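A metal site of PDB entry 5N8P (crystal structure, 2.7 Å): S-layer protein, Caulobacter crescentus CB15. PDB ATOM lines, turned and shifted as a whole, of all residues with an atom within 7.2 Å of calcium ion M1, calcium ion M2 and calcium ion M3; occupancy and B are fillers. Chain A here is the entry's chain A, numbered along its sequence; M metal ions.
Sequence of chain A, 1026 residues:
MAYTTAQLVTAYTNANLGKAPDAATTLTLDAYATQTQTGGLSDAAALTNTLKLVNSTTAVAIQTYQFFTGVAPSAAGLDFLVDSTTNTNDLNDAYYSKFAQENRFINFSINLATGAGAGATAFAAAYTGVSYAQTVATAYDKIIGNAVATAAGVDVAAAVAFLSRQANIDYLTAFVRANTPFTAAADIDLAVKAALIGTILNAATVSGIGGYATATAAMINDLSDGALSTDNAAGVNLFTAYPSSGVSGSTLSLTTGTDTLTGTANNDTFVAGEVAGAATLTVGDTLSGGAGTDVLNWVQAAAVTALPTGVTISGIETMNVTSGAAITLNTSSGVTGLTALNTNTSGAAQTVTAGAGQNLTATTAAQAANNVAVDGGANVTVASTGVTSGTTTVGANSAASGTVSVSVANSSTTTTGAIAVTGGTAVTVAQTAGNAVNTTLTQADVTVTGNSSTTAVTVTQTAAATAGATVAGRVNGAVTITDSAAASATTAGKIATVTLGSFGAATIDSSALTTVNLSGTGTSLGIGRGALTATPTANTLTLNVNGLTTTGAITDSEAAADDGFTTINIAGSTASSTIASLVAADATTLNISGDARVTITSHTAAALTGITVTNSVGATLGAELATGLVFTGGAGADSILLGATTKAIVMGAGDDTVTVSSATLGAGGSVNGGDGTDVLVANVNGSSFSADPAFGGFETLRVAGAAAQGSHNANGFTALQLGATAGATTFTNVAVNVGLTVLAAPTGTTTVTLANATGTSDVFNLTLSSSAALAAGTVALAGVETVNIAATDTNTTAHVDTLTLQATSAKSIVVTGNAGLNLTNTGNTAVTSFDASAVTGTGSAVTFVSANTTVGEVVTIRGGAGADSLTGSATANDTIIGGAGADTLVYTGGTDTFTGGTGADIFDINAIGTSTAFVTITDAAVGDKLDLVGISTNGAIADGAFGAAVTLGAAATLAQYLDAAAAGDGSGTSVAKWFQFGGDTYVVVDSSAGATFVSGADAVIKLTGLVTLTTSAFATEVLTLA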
ATOM      1  N   SER A 844      20.414   2.818 -27.520  1.00  0.00           N
ATOM      2  CA  SER A 844      21.552   3.253 -28.333  1.00  0.00           C
ATOM      3  C   SER A 844      22.025   4.701 -27.974  1.00  0.00           C
ATOM      4  O   SER A 844      21.790   5.712 -28.680  1.00  0.00           O
ATOM      5  CB  SER A 844      21.405   2.966 -29.858  1.00  0.00           C
ATOM      6  OG  SER A 844      20.105   2.855 -30.400  1.00  0.00           O
ATOM      7  N   VAL A 846      23.964   8.017 -27.200  1.00  0.00           N
ATOM      8  CA  VAL A 846      24.979   8.823 -27.862  1.00  0.00           C
ATOM      9  C   VAL A 846      25.575   9.840 -26.904  1.00  0.00           C
ATOM     10  O   VAL A 846      24.846  10.567 -26.249  1.00  0.00           O
ATOM     11  CB  VAL A 846      24.384   9.485 -29.113  1.00  0.00           C
ATOM     12  CG1 VAL A 846      25.374  10.450 -29.755  1.00  0.00           C
ATOM     13  CG2 VAL A 846      23.888   8.415 -30.102  1.00  0.00           C
ATOM     14  N   ARG A 862      22.055  17.196 -32.104  1.00  0.00           N
ATOM     15  CA  ARG A 862      20.874  16.315 -32.156  1.00  0.00           C
ATOM     16  C   ARG A 862      21.105  14.905 -31.588  1.00  0.00           C
ATOM     17  O   ARG A 862      21.929  14.177 -32.113  1.00  0.00           O
ATOM     18  CB  ARG A 862      20.380  16.205 -33.605  1.00  0.00           C
ATOM     19  CG  ARG A 862      18.978  16.691 -33.844  1.00  0.00           C
ATOM     20  CD  ARG A 862      19.019  18.138 -34.247  1.00  0.00           C
ATOM     21  NE  ARG A 862      19.368  18.405 -35.658  1.00  0.00           N
ATOM     22  CZ  ARG A 862      18.479  18.742 -36.604  1.00  0.00           C
ATOM     23  NH1 ARG A 862      18.878  18.918 -37.848  1.00  0.00           N
ATOM     24  NH2 ARG A 862      17.191  18.934 -36.310  1.00  0.00           N
ATOM     25  N   GLY A 863      20.364  14.519 -30.568  1.00  0.00           N
ATOM     26  CA  GLY A 863      20.356  13.157 -30.026  1.00  0.00           C
ATOM     27  C   GLY A 863      19.431  12.198 -30.775  1.00  0.00           C
ATOM     28  O   GLY A 863      18.676  12.592 -31.681  1.00  0.00           O
ATOM     29  N   GLY A 864      19.499  10.920 -30.396  1.00  0.00           N
ATOM     30  CA  GLY A 864      18.724   9.850 -31.027  1.00  0.00           C
ATOM     31  C   GLY A 864      17.738   9.211 -30.082  1.00  0.00           C
ATOM     32  O   GLY A 864      17.308   9.848 -29.122  1.00  0.00           O
ATOM     33  N   ALA A 865      17.340   7.976 -30.343  1.00  0.00           N
ATOM     34  CA  ALA A 865      16.369   7.294 -29.480  1.00  0.00           C
ATOM     35  C   ALA A 865      16.941   6.940 -28.081  1.00  0.00           C
ATOM     36  O   ALA A 865      16.191   6.703 -27.141  1.00  0.00           O
ATOM     37  CB  ALA A 865      15.778   6.094 -30.169  1.00  0.00           C
ATOM     38  N   GLY A 866      18.260   6.947 -27.932  1.00  0.00           N
ATOM     39  CA  GLY A 866      18.926   6.516 -26.696  1.00  0.00           C
ATOM     40  C   GLY A 866      18.942   7.565 -25.612  1.00  0.00           C
ATOM     41  O   GLY A 866      18.584   8.696 -25.833  1.00  0.00           O
ATOM     42  N   ALA A 867      19.347   7.135 -24.429  1.00  0.00           N
ATOM     43  CA  ALA A 867      19.506   8.044 -23.280  1.00  0.00           C
ATOM     44  C   ALA A 867      20.809   8.822 -23.510  1.00  0.00           C
ATOM     45  O   ALA A 867      21.878   8.391 -23.035  1.00  0.00           O
ATOM     46  CB  ALA A 867      19.546   7.249 -21.959  1.00  0.00           C
ATOM     47  N   ASP A 868      20.723   9.940 -24.235  1.00  0.00           N
ATOM     48  CA  ASP A 868      21.933  10.628 -24.761  1.00  0.00           C
ATOM     49  C   ASP A 868      22.534  11.677 -23.799  1.00  0.00           C
ATOM     50  O   ASP A 868      21.862  12.174 -22.896  1.00  0.00           O
ATOM     51  CB  ASP A 868      21.676  11.269 -26.131  1.00  0.00           C
ATOM     52  CG  ASP A 868      20.967  10.326 -27.114  1.00  0.00           C
ATOM     53  OD1 ASP A 868      21.451   9.206 -27.465  1.00  0.00           O
ATOM     54  OD2 ASP A 868      19.883  10.719 -27.560  1.00  0.00           O
ATOM     55  N   SER A 869      23.810  12.019 -24.015  1.00  0.00           N
ATOM     56  CA  SER A 869      24.501  12.976 -23.160  1.00  0.00           C
ATOM     57  C   SER A 869      25.249  14.039 -23.974  1.00  0.00           C
ATOM     58  O   SER A 869      26.428  13.892 -24.331  1.00  0.00           O
ATOM     59  CB  SER A 869      25.415  12.267 -22.162  1.00  0.00           C
ATOM     60  OG  SER A 869      26.142  13.221 -21.411  1.00  0.00           O
ATOM     61  N   LEU A 870      24.535  15.131 -24.219  1.00  0.00           N
ATOM     62  CA  LEU A 870      24.925  16.150 -25.156  1.00  0.00           C
ATOM     63  C   LEU A 870      25.365  17.430 -24.438  1.00  0.00           C
ATOM     64  O   LEU A 870      24.572  18.040 -23.715  1.00  0.00           O
ATOM     65  CB  LEU A 870      23.742  16.402 -26.102  1.00  0.00           C
ATOM     66  CG  LEU A 870      22.986  15.165 -26.632  1.00  0.00           C
ATOM     67  CD1 LEU A 870      21.720  15.535 -27.354  1.00  0.00           C
ATOM     68  CD2 LEU A 870      23.861  14.308 -27.521  1.00  0.00           C
ATOM     69  N   ILE A 881      19.044  19.090 -28.955  1.00  0.00           N
ATOM     70  CA  ILE A 881      17.773  18.363 -29.038  1.00  0.00           C
ATOM     71  C   ILE A 881      18.013  16.872 -28.783  1.00  0.00           C
ATOM     72  O   ILE A 881      18.589  16.219 -29.638  1.00  0.00           O
ATOM     73  CB  ILE A 881      17.102  18.562 -30.425  1.00  0.00           C
ATOM     74  CG1 ILE A 881      16.614  19.996 -30.580  1.00  0.00           C
ATOM     75  CG2 ILE A 881      15.947  17.610 -30.703  1.00  0.00           C
ATOM     76  CD1 ILE A 881      16.799  20.588 -31.941  1.00  0.00           C
ATOM     77  N   GLY A 882      17.609  16.335 -27.631  1.00  0.00           N
ATOM     78  CA  GLY A 882      17.572  14.850 -27.416  1.00  0.00           C
ATOM     79  C   GLY A 882      16.405  14.229 -28.186  1.00  0.00           C
ATOM     80  O   GLY A 882      15.502  14.925 -28.628  1.00  0.00           O
ATOM     81  N   GLY A 883      16.385  12.931 -28.359  1.00  0.00           N
ATOM     82  CA  GLY A 883      15.229  12.330 -29.075  1.00  0.00           C
ATOM     83  C   GLY A 883      14.174  11.807 -28.134  1.00  0.00           C
ATOM     84  O   GLY A 883      13.596  12.548 -27.356  1.00  0.00           O
ATOM     85  N   ALA A 884      13.924  10.500 -28.230  1.00  0.00           N
ATOM     86  CA  ALA A 884      13.259   9.727 -27.182  1.00  0.00           C
ATOM     87  C   ALA A 884      14.240   9.568 -26.004  1.00  0.00           C
ATOM     88  O   ALA A 884      15.383  10.041 -26.100  1.00  0.00           O
ATOM     89  CB  ALA A 884      12.772   8.381 -27.725  1.00  0.00           C
ATOM     90  N   GLY A 885      13.800   8.960 -24.876  1.00  0.00           N
ATOM     91  CA  GLY A 885      14.726   8.542 -23.806  1.00  0.00           C
ATOM     92  C   GLY A 885      15.344   9.611 -22.912  1.00  0.00           C
ATOM     93  O   GLY A 885      15.239  10.808 -23.174  1.00  0.00           O
ATOM     94  N   ALA A 886      15.986   9.153 -21.844  1.00  0.00           N
ATOM     95  CA  ALA A 886      16.438  10.003 -20.723  1.00  0.00           C
ATOM     96  C   ALA A 886      17.692  10.847 -21.066  1.00  0.00           C
ATOM     97  O   ALA A 886      18.820  10.492 -20.698  1.00  0.00           O
ATOM     98  CB  ALA A 886      16.663   9.150 -19.447  1.00  0.00           C
ATOM     99  N   ASP A 887      17.480  11.959 -21.767  1.00  0.00           N
ATOM    100  CA  ASP A 887      18.588  12.761 -22.271  1.00  0.00           C
ATOM    101  C   ASP A 887      19.118  13.711 -21.225  1.00  0.00           C
ATOM    102  O   ASP A 887      18.350  14.217 -20.402  1.00  0.00           O
ATOM    103  CB  ASP A 887      18.177  13.527 -23.515  1.00  0.00           C
ATOM    104  CG  ASP A 887      17.718  12.623 -24.636  1.00  0.00           C
ATOM    105  OD1 ASP A 887      18.536  11.772 -25.072  1.00  0.00           O
ATOM    106  OD2 ASP A 887      16.567  12.758 -25.090  1.00  0.00           O
ATOM    107  N   THR A 888      20.438  13.905 -21.223  1.00  0.00           N
ATOM    108  CA  THR A 888      21.092  14.938 -20.414  1.00  0.00           C
ATOM    109  C   THR A 888      21.641  16.025 -21.359  1.00  0.00           C
ATOM    110  O   THR A 888      22.486  15.731 -22.211  1.00  0.00           O
ATOM    111  CB  THR A 888      22.164  14.340 -19.454  1.00  0.00           C
ATOM    112  OG1 THR A 888      21.542  13.403 -18.567  1.00  0.00           O
ATOM    113  CG2 THR A 888      22.857  15.443 -18.586  1.00  0.00           C
ATOM    114  N   LEU A 889      21.126  17.243 -21.216  1.00  0.00           N
ATOM    115  CA  LEU A 889      21.526  18.383 -22.027  1.00  0.00           C
ATOM    116  C   LEU A 889      22.277  19.344 -21.130  1.00  0.00           C
ATOM    117  O   LEU A 889      21.747  19.792 -20.126  1.00  0.00           O
ATOM    118  CB  LEU A 889      20.280  19.041 -22.606  1.00  0.00           C
ATOM    119  CG  LEU A 889      19.602  18.404 -23.829  1.00  0.00           C
ATOM    120  CD1 LEU A 889      19.046  17.016 -23.584  1.00  0.00           C
ATOM    121  CD2 LEU A 889      18.494  19.305 -24.336  1.00  0.00           C
ATOM    122  N   THR A 899      15.805  21.281 -26.071  1.00  0.00           N
ATOM    123  CA  THR A 899      14.600  20.508 -26.288  1.00  0.00           C
ATOM    124  C   THR A 899      14.979  19.074 -25.971  1.00  0.00           C
ATOM    125  O   THR A 899      15.675  18.440 -26.756  1.00  0.00           O
ATOM    126  CB  THR A 899      14.113  20.641 -27.756  1.00  0.00           C
ATOM    127  OG1 THR A 899      13.944  22.023 -28.099  1.00  0.00           O
ATOM    128  CG2 THR A 899      12.823  19.867 -28.009  1.00  0.00           C
ATOM    129  N   GLY A 900      14.603  18.586 -24.798  1.00  0.00           N
ATOM    130  CA  GLY A 900      14.706  17.138 -24.545  1.00  0.00           C
ATOM    131  C   GLY A 900      13.370  16.692 -25.057  1.00  0.00           C
ATOM    132  O   GLY A 900      12.382  17.309 -24.680  1.00  0.00           O
ATOM    133  N   GLY A 901      13.291  15.693 -25.922  1.00  0.00           N
ATOM    134  CA  GLY A 901      12.002  15.296 -26.503  1.00  0.00           C
ATOM    135  C   GLY A 901      11.131  14.560 -25.493  1.00  0.00           C
ATOM    136  O   GLY A 901      10.909  15.016 -24.358  1.00  0.00           O
ATOM    137  N   THR A 902      10.643  13.403 -25.911  1.00  0.00           N
ATOM    138  CA  THR A 902       9.919  12.509 -25.016  1.00  0.00           C
ATOM    139  C   THR A 902      10.890  11.977 -23.924  1.00  0.00           C
ATOM    140  O   THR A 902      12.119  12.002 -24.117  1.00  0.00           O
ATOM    141  CB  THR A 902       9.241  11.375 -25.815  1.00  0.00           C
ATOM    142  OG1 THR A 902      10.223  10.402 -26.218  1.00  0.00           O
ATOM    143  CG2 THR A 902       8.542  11.913 -27.080  1.00  0.00           C
ATOM    144  N   GLY A 903      10.330  11.553 -22.783  1.00  0.00           N
ATOM    145  CA  GLY A 903      11.122  10.950 -21.707  1.00  0.00           C
ATOM    146  C   GLY A 903      11.590  11.889 -20.612  1.00  0.00           C
ATOM    147  O   GLY A 903      11.515  13.107 -20.747  1.00  0.00           O
ATOM    148  N   ALA A 904      12.065  11.297 -19.509  1.00  0.00           N
ATOM    149  CA  ALA A 904      12.531  12.021 -18.326  1.00  0.00           C
ATOM    150  C   ALA A 904      13.886  12.661 -18.600  1.00  0.00           C
ATOM    151  O   ALA A 904      14.934  12.096 -18.253  1.00  0.00           O
ATOM    152  CB  ALA A 904      12.610  11.058 -17.124  1.00  0.00           C
ATOM    153  N   ASP A 905      13.883  13.839 -19.232  1.00  0.00           N
ATOM    154  CA  ASP A 905      15.136  14.506 -19.585  1.00  0.00           C
ATOM    155  C   ASP A 905      15.707  15.283 -18.416  1.00  0.00           C
ATOM    156  O   ASP A 905      14.954  15.718 -17.555  1.00  0.00           O
ATOM    157  CB  ASP A 905      14.933  15.414 -20.796  1.00  0.00           C
ATOM    158  CG  ASP A 905      14.379  14.664 -21.983  1.00  0.00           C
ATOM    159  OD1 ASP A 905      15.106  13.827 -22.555  1.00  0.00           O
ATOM    160  OD2 ASP A 905      13.220  14.915 -22.334  1.00  0.00           O
ATOM    161  N   ILE A 906      17.021  15.398 -18.357  1.00  0.00           N
ATOM    162  CA  ILE A 906      17.640  16.206 -17.295  1.00  0.00           C
ATOM    163  C   ILE A 906      18.394  17.405 -17.931  1.00  0.00           C
ATOM    164  O   ILE A 906      19.238  17.227 -18.802  1.00  0.00           O
ATOM    165  CB  ILE A 906      18.356  15.348 -16.158  1.00  0.00           C
ATOM    166  CG1 ILE A 906      19.766  15.896 -15.758  1.00  0.00           C
ATOM    167  CG2 ILE A 906      18.316  13.821 -16.433  1.00  0.00           C
ATOM    168  CD1 ILE A 906      20.483  15.143 -14.625  1.00  0.00           C
ATOM    169  N   PHE A 907      17.996  18.632 -17.562  1.00  0.00           N
ATOM    170  CA  PHE A 907      18.643  19.844 -18.079  1.00  0.00           C
ATOM    171  C   PHE A 907      19.682  20.287 -17.067  1.00  0.00           C
ATOM    172  O   PHE A 907      19.341  20.937 -16.076  1.00  0.00           O
ATOM    173  CB  PHE A 907      17.623  20.934 -18.353  1.00  0.00           C
ATOM    174  CG  PHE A 907      16.551  20.497 -19.288  1.00  0.00           C
ATOM    175  CD1 PHE A 907      16.791  20.396 -20.659  1.00  0.00           C
ATOM    176  CD2 PHE A 907      15.291  20.143 -18.814  1.00  0.00           C
ATOM    177  CE1 PHE A 907      15.807  19.992 -21.540  1.00  0.00           C
ATOM    178  CE2 PHE A 907      14.288  19.723 -19.692  1.00  0.00           C
ATOM    179  CZ  PHE A 907      14.547  19.638 -21.066  1.00  0.00           C
ATOM    180  N   ASP A 923      10.512  22.799 -24.075  1.00  0.00           N
ATOM    181  CA  ASP A 923       9.415  21.841 -23.849  1.00  0.00           C
ATOM    182  C   ASP A 923       9.353  21.180 -22.483  1.00  0.00           C
ATOM    183  O   ASP A 923       8.818  20.058 -22.361  1.00  0.00           O
ATOM    184  CB  ASP A 923       9.426  20.760 -24.962  1.00  0.00           C
ATOM    185  CG  ASP A 923      10.669  19.844 -24.914  1.00  0.00           C
ATOM    186  OD1 ASP A 923      11.629  20.014 -24.079  1.00  0.00           O
ATOM    187  OD2 ASP A 923      10.657  18.936 -25.757  1.00  0.00           O
ATOM    188  N   ALA A 924       9.904  21.858 -21.475  1.00  0.00           N
ATOM    189  CA  ALA A 924       9.826  21.399 -20.077  1.00  0.00           C
ATOM    190  C   ALA A 924       8.416  20.875 -19.740  1.00  0.00           C
ATOM    191  O   ALA A 924       7.419  21.560 -19.943  1.00  0.00           O
ATOM    192  CB  ALA A 924      10.233  22.508 -19.128  1.00  0.00           C
ATOM    193  N   ALA A 925       8.371  19.634 -19.304  1.00  0.00           N
ATOM    194  CA  ALA A 925       7.112  18.938 -19.019  1.00  0.00           C
ATOM    195  C   ALA A 925       7.272  18.068 -17.780  1.00  0.00           C
ATOM    196  O   ALA A 925       8.381  17.896 -17.261  1.00  0.00           O
ATOM    197  CB  ALA A 925       6.658  18.103 -20.218  1.00  0.00           C
ATOM    198  N   VAL A 926       6.142  17.563 -17.293  1.00  0.00           N
ATOM    199  CA  VAL A 926       6.088  16.659 -16.163  1.00  0.00           C
ATOM    200  C   VAL A 926       7.072  15.475 -16.343  1.00  0.00           C
ATOM    201  O   VAL A 926       7.035  14.759 -17.363  1.00  0.00           O
ATOM    202  CB  VAL A 926       4.616  16.226 -15.895  1.00  0.00           C
ATOM    203  CG1 VAL A 926       3.978  15.527 -17.113  1.00  0.00           C
ATOM    204  CG2 VAL A 926       4.497  15.388 -14.622  1.00  0.00           C
ATOM    205  N   GLY A 927       7.974  15.317 -15.373  1.00  0.00           N
ATOM    206  CA  GLY A 927       8.981  14.244 -15.398  1.00  0.00           C
ATOM    207  C   GLY A 927      10.413  14.706 -15.653  1.00  0.00           C
ATOM    208  O   GLY A 927      11.358  14.129 -15.095  1.00  0.00           O
ATOM    209  N   ASP A 928      10.550  15.739 -16.485  1.00  0.00           N
ATOM    210  CA  ASP A 928      11.842  16.380 -16.736  1.00  0.00           C
ATOM    211  C   ASP A 928      12.422  17.007 -15.473  1.00  0.00           C
ATOM    212  O   ASP A 928      11.658  17.417 -14.588  1.00  0.00           O
ATOM    213  CB  ASP A 928      11.731  17.423 -17.862  1.00  0.00           C
ATOM    214  CG  ASP A 928      11.343  16.817 -19.226  1.00  0.00           C
ATOM    215  OD1 ASP A 928      10.537  17.425 -19.959  1.00  0.00           O
ATOM    216  OD2 ASP A 928      11.835  15.732 -19.601  1.00  0.00           O
HETATM  217 CA    CA M   1      14.303  12.925 -24.749  1.00  0.00          CA
HETATM  218 CA    CA M   2      17.666  10.784 -26.881  1.00  0.00          CA
HETATM  219 CA    CA M   3      10.950  15.208 -21.868  1.00  0.00          CA
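Merely in contact with calcium ion M3: Gly 900. Within 4 Å of calcium ion M3: Gly 900, Gly 901, Thr 902, Gly 903, Asp 905 and Asp 928.
Calcium ion M3 is bound by OD2 of Asp 905 (2.3 Å). O of Gly 903 binds calcium ion M3, 2.4 Å away. Calcium ion M3 is bound by the side-chain carboxylate (OD2) of Asp 928 (2.5 Å). Calcium ion M3 is bound by the backbone carbonyl oxygen (O) of Gly 901 (2.5 Å). Calcium ion M3 has four donor atoms within binding distance. Slightly farther from calcium ion M3 lies the side-chain carboxylate (OD1) of Asp 928 (3.0 Å).
Calcium ion M2 is bound by the side-chain carboxylate (OD1) of Asp 887 (2.2 Å), the side-chain carboxylate (OD2) of Asp 868 (2.3 Å), the backbone carbonyl oxygen (O) of Gly 864 (2.5 Å), the backbone carbonyl oxygen (O) of Gly 866 (2.5 Å), the backbone carbonyl oxygen (O) of Ala 884 (2.5 Å) and the side-chain carboxylate (OD2) of Asp 887 (2.9 Å). Calcium ion M2 has six donor atoms within binding distance. Slightly farther from calcium ion M2 lies the backbone nitrogen (N) of Gly 883 (2.9 Å).
Calcium ion M1 is bound by OD2 of Asp 887 (2.3 Å), O of Thr 902 (2.5 Å), OD1 of Asp 905 (2.5 Å), O of Gly 883 (2.7 Å) and O of Gly 885 (2.8 Å).
O of Asp 887 lies within hydrogen-bond range of N of Ile 906. The side-chain carboxylate (OD1) of Asp 868 sits at hydrogen-bond distance from the backbone NH (N) of Val 846, at 2.8 Å. The backbone carbonyl oxygen (O) of Asp 868 is in hydrogen-bond range of the backbone NH (N) of Thr 888 (2.8 Å). The backbone carbonyl oxygen (O) of Gly 864 sits close to the backbone NH (N) of Gly 883 (3.3 Å). N of Ala 925 is in hydrogen-bond range of OD1 of Asp 928. The backbone carbonyl oxygen (O) of Gly 883 lies close to the backbone NH (N) of Gly 901 (3.5 Å). The backbone NH (N) of Gly 900 is in hydrogen-bond range of the side-chain carboxylate (OD1) of Asp 923, at 3.4 Å. The backbone NH (N) of Gly 882 lies within hydrogen-bond range of the backbone carbonyl oxygen (O) of Thr 899, 3.0 Å away.
Residues that only touch calcium ion M1: Gly 900 (3.9 Å). Within 4 Å of calcium ion M1: Gly 883, Ala 884, Gly 885, Asp 887, Gly 900, Gly 901, Thr 902 and Asp 905.
Residues that only touch calcium ion M2: Gly 882. Seven residues have an atom within 4 Å of calcium ion M2: Gly 864, Gly 866, Asp 868, Gly 882, Gly 883, Ala 884 and Asp 887. Along chain A the residues within 4 Å of calcium ion M2 span positions 864 to 887.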
